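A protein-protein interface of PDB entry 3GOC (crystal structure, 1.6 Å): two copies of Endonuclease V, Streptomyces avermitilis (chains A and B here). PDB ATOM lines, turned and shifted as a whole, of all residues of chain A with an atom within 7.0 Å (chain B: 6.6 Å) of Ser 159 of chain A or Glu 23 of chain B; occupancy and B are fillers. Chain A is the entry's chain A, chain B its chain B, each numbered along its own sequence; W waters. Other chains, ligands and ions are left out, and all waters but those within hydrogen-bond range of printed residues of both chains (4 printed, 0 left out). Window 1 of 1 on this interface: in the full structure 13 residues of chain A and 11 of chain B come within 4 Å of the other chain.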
ATOM      1  N   PRO A 153     -21.371   4.645  18.739  1.00  0.00           N
ATOM      2  CA  PRO A 153     -20.202   4.230  17.960  1.00  0.00           C
ATOM      3  C   PRO A 153     -19.207   3.538  18.891  1.00  0.00           C
ATOM      4  O   PRO A 153     -19.389   3.548  20.110  1.00  0.00           O
ATOM      5  CB  PRO A 153     -19.661   5.553  17.417  1.00  0.00           C
ATOM      6  CG  PRO A 153     -20.018   6.524  18.498  1.00  0.00           C
ATOM      7  CD  PRO A 153     -21.430   6.111  18.860  1.00  0.00           C
ATOM      8  N   GLY A 154     -18.169   2.929  18.326  1.00  0.00           N
ATOM      9  CA  GLY A 154     -17.172   2.274  19.152  1.00  0.00           C
ATOM     10  C   GLY A 154     -16.634   3.257  20.174  1.00  0.00           C
ATOM     11  O   GLY A 154     -16.689   4.474  19.973  1.00  0.00           O
ATOM     12  N   ALA A 155     -16.111   2.739  21.279  1.00  0.00           N
ATOM     13  CA  ALA A 155     -15.568   3.592  22.333  1.00  0.00           C
ATOM     14  C   ALA A 155     -14.282   4.340  21.968  1.00  0.00           C
ATOM     15  O   ALA A 155     -14.088   5.480  22.380  1.00  0.00           O
ATOM     16  CB  ALA A 155     -15.350   2.764  23.599  1.00  0.00           C
ATOM     17  N   PRO A 156     -13.381   3.708  21.198  1.00  0.00           N
ATOM     18  CA  PRO A 156     -12.142   4.410  20.844  1.00  0.00           C
ATOM     19  C   PRO A 156     -12.328   5.618  19.935  1.00  0.00           C
ATOM     20  O   PRO A 156     -13.236   5.649  19.106  1.00  0.00           O
ATOM     21  CB  PRO A 156     -11.307   3.326  20.163  1.00  0.00           C
ATOM     22  CG  PRO A 156     -11.832   2.047  20.778  1.00  0.00           C
ATOM     23  CD  PRO A 156     -13.316   2.293  20.795  1.00  0.00           C
ATOM     24  N   ARG A 157     -11.459   6.612  20.104  1.00  0.00           N
ATOM     25  CA  ARG A 157     -11.486   7.800  19.263  1.00  0.00           C
ATOM     26  C   ARG A 157     -11.337   7.325  17.819  1.00  0.00           C
ATOM     27  O   ARG A 157     -10.551   6.418  17.532  1.00  0.00           O
ATOM     28  CB  ARG A 157     -10.328   8.735  19.639  1.00  0.00           C
ATOM     29  CG  ARG A 157      -9.956   9.803  18.593  1.00  0.00           C
ATOM     30  CD  ARG A 157      -8.913  10.770  19.178  1.00  0.00           C
ATOM     31  NE  ARG A 157      -8.115  11.483  18.180  1.00  0.00           N
ATOM     32  CZ  ARG A 157      -8.522  12.541  17.484  1.00  0.00           C
ATOM     33  NH1 ARG A 157      -7.703  13.112  16.603  1.00  0.00           N
ATOM     34  NH2 ARG A 157      -9.737  13.039  17.664  1.00  0.00           N
ATOM     35  N   GLY A 158     -12.095   7.935  16.914  1.00  0.00           N
ATOM     36  CA  GLY A 158     -12.037   7.544  15.516  1.00  0.00           C
ATOM     37  C   GLY A 158     -13.246   6.719  15.106  1.00  0.00           C
ATOM     38  O   GLY A 158     -13.601   6.659  13.926  1.00  0.00           O
ATOM     39  N   SER A 159     -13.872   6.076  16.086  1.00  0.00           N
ATOM     40  CA  SER A 159     -15.055   5.256  15.852  1.00  0.00           C
ATOM     41  C   SER A 159     -16.222   6.115  15.372  1.00  0.00           C
ATOM     42  O   SER A 159     -16.387   7.258  15.803  1.00  0.00           O
ATOM     43  CB  SER A 159     -15.469   4.542  17.141  1.00  0.00           C
ATOM     44  OG  SER A 159     -14.429   3.720  17.639  1.00  0.00           O
ATOM     45  N   ALA A 160     -17.041   5.553  14.493  1.00  0.00           N
ATOM     46  CA  ALA A 160     -18.186   6.270  13.969  1.00  0.00           C
ATOM     47  C   ALA A 160     -19.393   5.352  13.863  1.00  0.00           C
ATOM     48  O   ALA A 160     -19.283   4.128  13.975  1.00  0.00           O
ATOM     49  CB  ALA A 160     -17.850   6.851  12.592  1.00  0.00           C
ATOM     50  N   ALA A 161     -20.551   5.958  13.652  1.00  0.00           N
ATOM     51  CA  ALA A 161     -21.790   5.215  13.488  1.00  0.00           C
ATOM     52  C   ALA A 161     -22.711   6.097  12.663  1.00  0.00           C
ATOM     53  O   ALA A 161     -22.628   7.320  12.717  1.00  0.00           O
ATOM     54  CB  ALA A 161     -22.413   4.917  14.846  1.00  0.00           C
ATOM     55  N   ALA A 173     -22.169   9.808  13.784  1.00  0.00           N
ATOM     56  CA  ALA A 173     -21.846  10.159  15.156  1.00  0.00           C
ATOM     57  C   ALA A 173     -20.368   9.760  15.167  1.00  0.00           C
ATOM     58  O   ALA A 173     -20.020   8.631  14.810  1.00  0.00           O
ATOM     59  CB  ALA A 173     -22.643   9.311  16.130  1.00  0.00           C
ATOM     60  N   LEU A 174     -19.497  10.689  15.546  1.00  0.00           N
ATOM     61  CA  LEU A 174     -18.061  10.433  15.536  1.00  0.00           C
ATOM     62  C   LEU A 174     -17.424  10.602  16.901  1.00  0.00           C
ATOM     63  O   LEU A 174     -17.593  11.636  17.546  1.00  0.00           O
ATOM     64  CB  LEU A 174     -17.384  11.393  14.554  1.00  0.00           C
ATOM     65  CG  LEU A 174     -15.865  11.292  14.412  1.00  0.00           C
ATOM     66  CD1 LEU A 174     -15.504   9.974  13.738  1.00  0.00           C
ATOM     67  CD2 LEU A 174     -15.351  12.466  13.581  1.00  0.00           C
ATOM     68  N   ARG A 175     -16.688   9.583  17.333  1.00  0.00           N
ATOM     69  CA  ARG A 175     -16.006   9.620  18.618  1.00  0.00           C
ATOM     70  C   ARG A 175     -14.726  10.430  18.431  1.00  0.00           C
ATOM     71  O   ARG A 175     -13.761   9.935  17.846  1.00  0.00           O
ATOM     72  CB  ARG A 175     -15.657   8.191  19.070  1.00  0.00           C
ATOM     73  CG  ARG A 175     -15.139   8.101  20.500  1.00  0.00           C
ATOM     74  CD  ARG A 175     -16.281   8.161  21.509  1.00  0.00           C
ATOM     75  NE  ARG A 175     -17.131   6.969  21.443  1.00  0.00           N
ATOM     76  CZ  ARG A 175     -18.223   6.782  22.179  1.00  0.00           C
ATOM     77  NH1 ARG A 175     -18.613   7.708  23.045  1.00  0.00           N
ATOM     78  NH2 ARG A 175     -18.939   5.672  22.048  1.00  0.00           N
ATOM     79  N   THR A 176     -14.715  11.675  18.905  1.00  0.00           N
ATOM     80  CA  THR A 176     -13.528  12.519  18.773  1.00  0.00           C
ATOM     81  C   THR A 176     -12.608  12.355  19.973  1.00  0.00           C
ATOM     82  O   THR A 176     -11.414  12.623  19.887  1.00  0.00           O
ATOM     83  CB  THR A 176     -13.910  14.010  18.596  1.00  0.00           C
ATOM     84  OG1 THR A 176     -14.864  14.383  19.600  1.00  0.00           O
ATOM     85  CG2 THR A 176     -14.516  14.242  17.214  1.00  0.00           C
ATOM     86  N   PRO A 182     -19.873  11.371  21.608  1.00  0.00           N
ATOM     87  CA  PRO A 182     -19.453  11.772  20.259  1.00  0.00           C
ATOM     88  C   PRO A 182     -20.047  13.091  19.776  1.00  0.00           C
ATOM     89  O   PRO A 182     -20.911  13.684  20.438  1.00  0.00           O
ATOM     90  CB  PRO A 182     -19.912  10.604  19.393  1.00  0.00           C
ATOM     91  CG  PRO A 182     -21.163  10.147  20.095  1.00  0.00           C
ATOM     92  CD  PRO A 182     -20.767  10.197  21.556  1.00  0.00           C
ATOM     93  N   CYS A 197     -15.198  13.317   8.364  1.00  0.00           N
ATOM     94  CA  CYS A 197     -14.754  12.700   9.606  1.00  0.00           C
ATOM     95  C   CYS A 197     -13.261  12.914   9.816  1.00  0.00           C
ATOM     96  O   CYS A 197     -12.818  13.206  10.928  1.00  0.00           O
ATOM     97  CB  CYS A 197     -15.054  11.206   9.595  1.00  0.00           C
ATOM     98  SG  CYS A 197     -16.791  10.836   9.841  1.00  0.00           S
ATOM     99  N   LEU A 201     -11.613  14.761  13.020  1.00  0.00           N
ATOM    100  CA  LEU A 201     -10.633  14.126  13.908  1.00  0.00           C
ATOM    101  C   LEU A 201      -9.357  14.964  13.962  1.00  0.00           C
ATOM    102  O   LEU A 201      -8.776  15.157  15.029  1.00  0.00           O
ATOM    103  CB  LEU A 201     -10.289  12.711  13.430  1.00  0.00           C
ATOM    104  CG  LEU A 201     -11.384  11.647  13.556  1.00  0.00           C
ATOM    105  CD1 LEU A 201     -10.868  10.331  12.987  1.00  0.00           C
ATOM    106  CD2 LEU A 201     -11.785  11.477  15.025  1.00  0.00           C
ATOM    107  N   ARG B  18     -10.773  -6.429  16.635  1.00  0.00           N
ATOM    108  CA  ARG B  18     -11.045  -6.712  15.233  1.00  0.00           C
ATOM    109  C   ARG B  18     -12.141  -5.787  14.717  1.00  0.00           C
ATOM    110  O   ARG B  18     -12.151  -5.423  13.539  1.00  0.00           O
ATOM    111  CB  ARG B  18     -11.476  -8.170  15.041  1.00  0.00           C
ATOM    112  CG  ARG B  18     -10.453  -9.190  15.508  1.00  0.00           C
ATOM    113  CD  ARG B  18     -10.930 -10.614  15.265  1.00  0.00           C
ATOM    114  NE  ARG B  18     -10.070 -11.591  15.929  1.00  0.00           N
ATOM    115  CZ  ARG B  18      -8.792 -11.792  15.625  1.00  0.00           C
ATOM    116  NH1 ARG B  18      -8.216 -11.085  14.660  1.00  0.00           N
ATOM    117  NH2 ARG B  18      -8.084 -12.691  16.293  1.00  0.00           N
ATOM    118  N   ALA B  19     -13.064  -5.408  15.598  1.00  0.00           N
ATOM    119  CA  ALA B  19     -14.156  -4.514  15.212  1.00  0.00           C
ATOM    120  C   ALA B  19     -13.572  -3.169  14.794  1.00  0.00           C
ATOM    121  O   ALA B  19     -14.004  -2.582  13.805  1.00  0.00           O
ATOM    122  CB  ALA B  19     -15.121  -4.328  16.376  1.00  0.00           C
ATOM    123  N   VAL B  20     -12.596  -2.688  15.558  1.00  0.00           N
ATOM    124  CA  VAL B  20     -11.937  -1.424  15.250  1.00  0.00           C
ATOM    125  C   VAL B  20     -11.226  -1.542  13.907  1.00  0.00           C
ATOM    126  O   VAL B  20     -11.328  -0.654  13.058  1.00  0.00           O
ATOM    127  CB  VAL B  20     -10.902  -1.049  16.343  1.00  0.00           C
ATOM    128  CG1 VAL B  20     -10.057   0.149  15.897  1.00  0.00           C
ATOM    129  CG2 VAL B  20     -11.619  -0.722  17.639  1.00  0.00           C
ATOM    130  N   GLN B  21     -10.507  -2.642  13.705  1.00  0.00           N
ATOM    131  CA  GLN B  21      -9.794  -2.833  12.444  1.00  0.00           C
ATOM    132  C   GLN B  21     -10.749  -2.889  11.256  1.00  0.00           C
ATOM    133  O   GLN B  21     -10.530  -2.223  10.246  1.00  0.00           O
ATOM    134  CB  GLN B  21      -8.961  -4.118  12.473  1.00  0.00           C
ATOM    135  CG  GLN B  21      -7.897  -4.156  13.555  1.00  0.00           C
ATOM    136  CD  GLN B  21      -7.020  -5.386  13.437  1.00  0.00           C
ATOM    137  OE1 GLN B  21      -7.516  -6.494  13.248  1.00  0.00           O
ATOM    138  NE2 GLN B  21      -5.711  -5.200  13.569  1.00  0.00           N
ATOM    139  N   ASP B  22     -11.808  -3.683  11.371  1.00  0.00           N
ATOM    140  CA  ASP B  22     -12.757  -3.802  10.276  1.00  0.00           C
ATOM    141  C   ASP B  22     -13.478  -2.500   9.975  1.00  0.00           C
ATOM    142  O   ASP B  22     -13.946  -2.291   8.856  1.00  0.00           O
ATOM    143  CB  ASP B  22     -13.773  -4.907  10.562  1.00  0.00           C
ATOM    144  CG  ASP B  22     -13.185  -6.292  10.377  1.00  0.00           C
ATOM    145  OD1 ASP B  22     -12.453  -6.489   9.380  1.00  0.00           O
ATOM    146  OD2 ASP B  22     -13.463  -7.183  11.213  1.00  0.00           O
ATOM    147  N   GLU B  23     -13.572  -1.618  10.963  1.00  0.00           N
ATOM    148  CA  GLU B  23     -14.242  -0.349  10.735  1.00  0.00           C
ATOM    149  C   GLU B  23     -13.314   0.688  10.117  1.00  0.00           C
ATOM    150  O   GLU B  23     -13.685   1.368   9.160  1.00  0.00           O
ATOM    151  CB  GLU B  23     -14.805   0.220  12.034  1.00  0.00           C
ATOM    152  CG  GLU B  23     -15.470   1.564  11.813  1.00  0.00           C
ATOM    153  CD  GLU B  23     -15.775   2.313  13.093  1.00  0.00           C
ATOM    154  OE1 GLU B  23     -16.289   3.439  12.985  1.00  0.00           O
ATOM    155  OE2 GLU B  23     -15.505   1.783  14.190  1.00  0.00           O
ATOM    156  N   LEU B  24     -12.110   0.811  10.667  1.00  0.00           N
ATOM    157  CA  LEU B  24     -11.149   1.794  10.176  1.00  0.00           C
ATOM    158  C   LEU B  24     -10.454   1.405   8.873  1.00  0.00           C
ATOM    159  O   LEU B  24     -10.015   2.276   8.118  1.00  0.00           O
ATOM    160  CB  LEU B  24     -10.092   2.080  11.249  1.00  0.00           C
ATOM    161  CG  LEU B  24     -10.581   2.610  12.600  1.00  0.00           C
ATOM    162  CD1 LEU B  24      -9.387   2.925  13.482  1.00  0.00           C
ATOM    163  CD2 LEU B  24     -11.435   3.855  12.398  1.00  0.00           C
ATOM    164  N   ARG B  25     -10.351   0.107   8.602  1.00  0.00           N
ATOM    165  CA  ARG B  25      -9.689  -0.356   7.385  1.00  0.00           C
ATOM    166  C   ARG B  25     -10.314   0.243   6.127  1.00  0.00           C
ATOM    167  O   ARG B  25      -9.618   0.496   5.142  1.00  0.00           O
ATOM    168  CB  ARG B  25      -9.743  -1.884   7.291  1.00  0.00           C
ATOM    169  CG  ARG B  25     -11.157  -2.427   7.191  1.00  0.00           C
ATOM    170  CD  ARG B  25     -11.213  -3.703   6.372  1.00  0.00           C
ATOM    171  NE  ARG B  25     -10.662  -4.856   7.071  1.00  0.00           N
ATOM    172  CZ  ARG B  25     -10.456  -6.038   6.499  1.00  0.00           C
ATOM    173  NH1 ARG B  25     -10.753  -6.213   5.218  1.00  0.00           N
ATOM    174  NH2 ARG B  25      -9.962  -7.048   7.208  1.00  0.00           N
ATOM    175  N   GLY B  26     -11.622   0.468   6.165  1.00  0.00           N
ATOM    176  CA  GLY B  26     -12.314   1.022   5.010  1.00  0.00           C
ATOM    177  C   GLY B  26     -12.015   2.486   4.770  1.00  0.00           C
ATOM    178  O   GLY B  26     -12.334   3.032   3.713  1.00  0.00           O
ATOM    179  N   ARG B  27     -11.393   3.127   5.752  1.00  0.00           N
ATOM    180  CA  ARG B  27     -11.057   4.537   5.632  1.00  0.00           C
ATOM    181  C   ARG B  27      -9.596   4.767   5.240  1.00  0.00           C
ATOM    182  O   ARG B  27      -9.123   5.902   5.177  1.00  0.00           O
ATOM    183  CB  ARG B  27     -11.436   5.254   6.936  1.00  0.00           C
ATOM    184  CG  ARG B  27     -12.942   5.518   7.016  1.00  0.00           C
ATOM    185  CD  ARG B  27     -13.499   5.562   8.436  1.00  0.00           C
ATOM    186  NE  ARG B  27     -12.939   6.632   9.252  1.00  0.00           N
ATOM    187  CZ  ARG B  27     -13.172   6.761  10.555  1.00  0.00           C
ATOM    188  NH1 ARG B  27     -13.958   5.889  11.178  1.00  0.00           N
ATOM    189  NH2 ARG B  27     -12.608   7.748  11.238  1.00  0.00           N
ATOM    190  N   PHE B 124      -4.436  -4.216   7.938  1.00  0.00           N
ATOM    191  CA  PHE B 124      -4.539  -2.989   8.714  1.00  0.00           C
ATOM    192  C   PHE B 124      -3.485  -2.968   9.814  1.00  0.00           C
ATOM    193  O   PHE B 124      -3.800  -3.039  11.002  1.00  0.00           O
ATOM    194  CB  PHE B 124      -5.941  -2.877   9.319  1.00  0.00           C
ATOM    195  CG  PHE B 124      -6.276  -1.502   9.817  1.00  0.00           C
ATOM    196  CD1 PHE B 124      -6.483  -1.267  11.169  1.00  0.00           C
ATOM    197  CD2 PHE B 124      -6.387  -0.439   8.929  1.00  0.00           C
ATOM    198  CE1 PHE B 124      -6.798   0.012  11.630  1.00  0.00           C
ATOM    199  CE2 PHE B 124      -6.699   0.840   9.379  1.00  0.00           C
ATOM    200  CZ  PHE B 124      -6.906   1.067  10.729  1.00  0.00           C
ATOM    201  N   LEU B 133      -6.015   7.212  12.221  1.00  0.00           N
ATOM    202  CA  LEU B 133      -6.234   7.956  13.454  1.00  0.00           C
ATOM    203  C   LEU B 133      -5.702   9.389  13.443  1.00  0.00           C
ATOM    204  O   LEU B 133      -6.274  10.260  14.089  1.00  0.00           O
ATOM    205  CB  LEU B 133      -5.638   7.195  14.640  1.00  0.00           C
ATOM    206  CG  LEU B 133      -6.361   5.900  15.023  1.00  0.00           C
ATOM    207  CD1 LEU B 133      -5.652   5.263  16.211  1.00  0.00           C
ATOM    208  CD2 LEU B 133      -7.823   6.195  15.375  1.00  0.00           C
HETATM  209  O   HOH W   1     -18.018   2.370  15.570  1.00  0.00           O
HETATM  210  O   HOH W   2     -13.287   2.103  15.831  1.00  0.00           O
HETATM  211  O   HOH W   3      -6.905  12.813  13.228  1.00  0.00           O
HETATM  212  O   HOH W   4      -5.891  10.047  16.896  1.00  0.00           O
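The side-chain carboxylate (OE1) of Glu 23 of chain B is in salt-bridge range of the guanidinium group (NH1) of Arg 27 of chain B.
N of Gly 158 of chain A lies within hydrogen-bond range of O of Arg 175 of chain A (2.8 Å).
The backbone carbonyl oxygen of Gly 154 of chain A sits close to the side-chain hydroxyl of Ser 159 of chain A (3.3 Å).
The backbone carbonyl oxygen of Thr 176 of chain A is in hydrogen-bond range of the guanidinium group of Arg 157 of chain A (2.8 Å).
The guanidinium group of Arg 157 of chain A sits at hydrogen-bond distance from the backbone carbonyl oxygen of Leu 201 of chain A, at 2.8 Å.
The backbone carbonyl oxygen (O) of Ser 159 of chain A sits at hydrogen-bond distance from the backbone NH (N) of Arg 175 of chain A, 2.8 Å away.
No position is printed for both chains.
Of the 6 pairs that touch across the chains among the printed residues, none has its exchanged pair printed and touching as well.
Of the 12 printed residues of chain B, 4 touch a printed residue of chain A.
Printed residues of chain B that touch a printed residue of chain A: Glu 23, Leu 24, Arg 27 and Leu 133.
Hydrophobic or aromatic side chains of chain A within 4 Å of the printed part of chain B: Ala 160 and Leu 201.
Among the printed residues, 6 pairs touch across the chains.
Among the printed residues, no Asp or Glu carboxylate lies within 4 Å of a Lys or Arg side-chain nitrogen of the other chain.
Of the printed residues of chain B, Gly 158 of chain A touches Leu 24 and Arg 27.
Of chain B, only Glu 23 (3.6 Å) comes within 4 Å of Ser 159 of chain A.
Printed residues of chain B within 4 Å of Ala 160 of chain A: Glu 23 (2.7 Å).
Val 20 of chain B touches none of the printed residues of chain A.
Of the printed residues of chain A, Leu 24 of chain B touches Gly 158 (3.9 Å).
Printed residues of chain A within 4 Å of Arg 27 of chain B: Gly 158 and Leu 201.
Of the printed residues of chain A, Leu 133 of chain B touches Arg 157 (3.5 Å).
The nearest residue of chain A that does not touch Glu 23 of chain B is Gly 158 of chain A (4.3 Å).
Arg 157 of chain A touches Leu 133 of chain B (O to CD2, 3.5 Å).
Gly 158 of chain A touches Leu 24 of chain B.
Ser 159 of chain A touches Glu 23 of chain B.
CD1 of Leu 201 of chain A touches NH2 of Arg 27 of chain B, 3.6 Å away.
The guanidinium group (NH1) of Arg 27 of chain B lies within hydrogen-bond range of the backbone carbonyl oxygen (O) of Gly 158 of chain A.
The backbone NH (N) of Ala 160 of chain A lies within hydrogen-bond range of the side-chain carboxylate (OE1) of Glu 23 of chain B, at 2.7 Å.
Water W2 lies within hydrogen-bond range of the side-chain hydroxyl of Ser 159 of chain A (2.7 Å) and the side-chain carboxylate of Glu 23 of chain B (2.8 Å).
Water W1 lies within hydrogen-bond range of O of Ala 160 of chain A (2.7 Å), N of Gly 154 of chain A (2.8 Å) and OE2 of Glu 23 of chain B (2.9 Å).
Water W3 lies within hydrogen-bond range of the backbone carbonyl oxygen (O) of Leu 133 of chain B (2.8 Å), the guanidinium group (NH1) of Arg 157 of chain A (3.5 Å) and the backbone carbonyl oxygen (O) of Leu 201 of chain A (3.5 Å).
Water W4 bridges the backbone carbonyl oxygen of Leu 133 of chain B (2.8 Å) and the guanidinium group of Arg 157 of chain A (2.9 Å).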
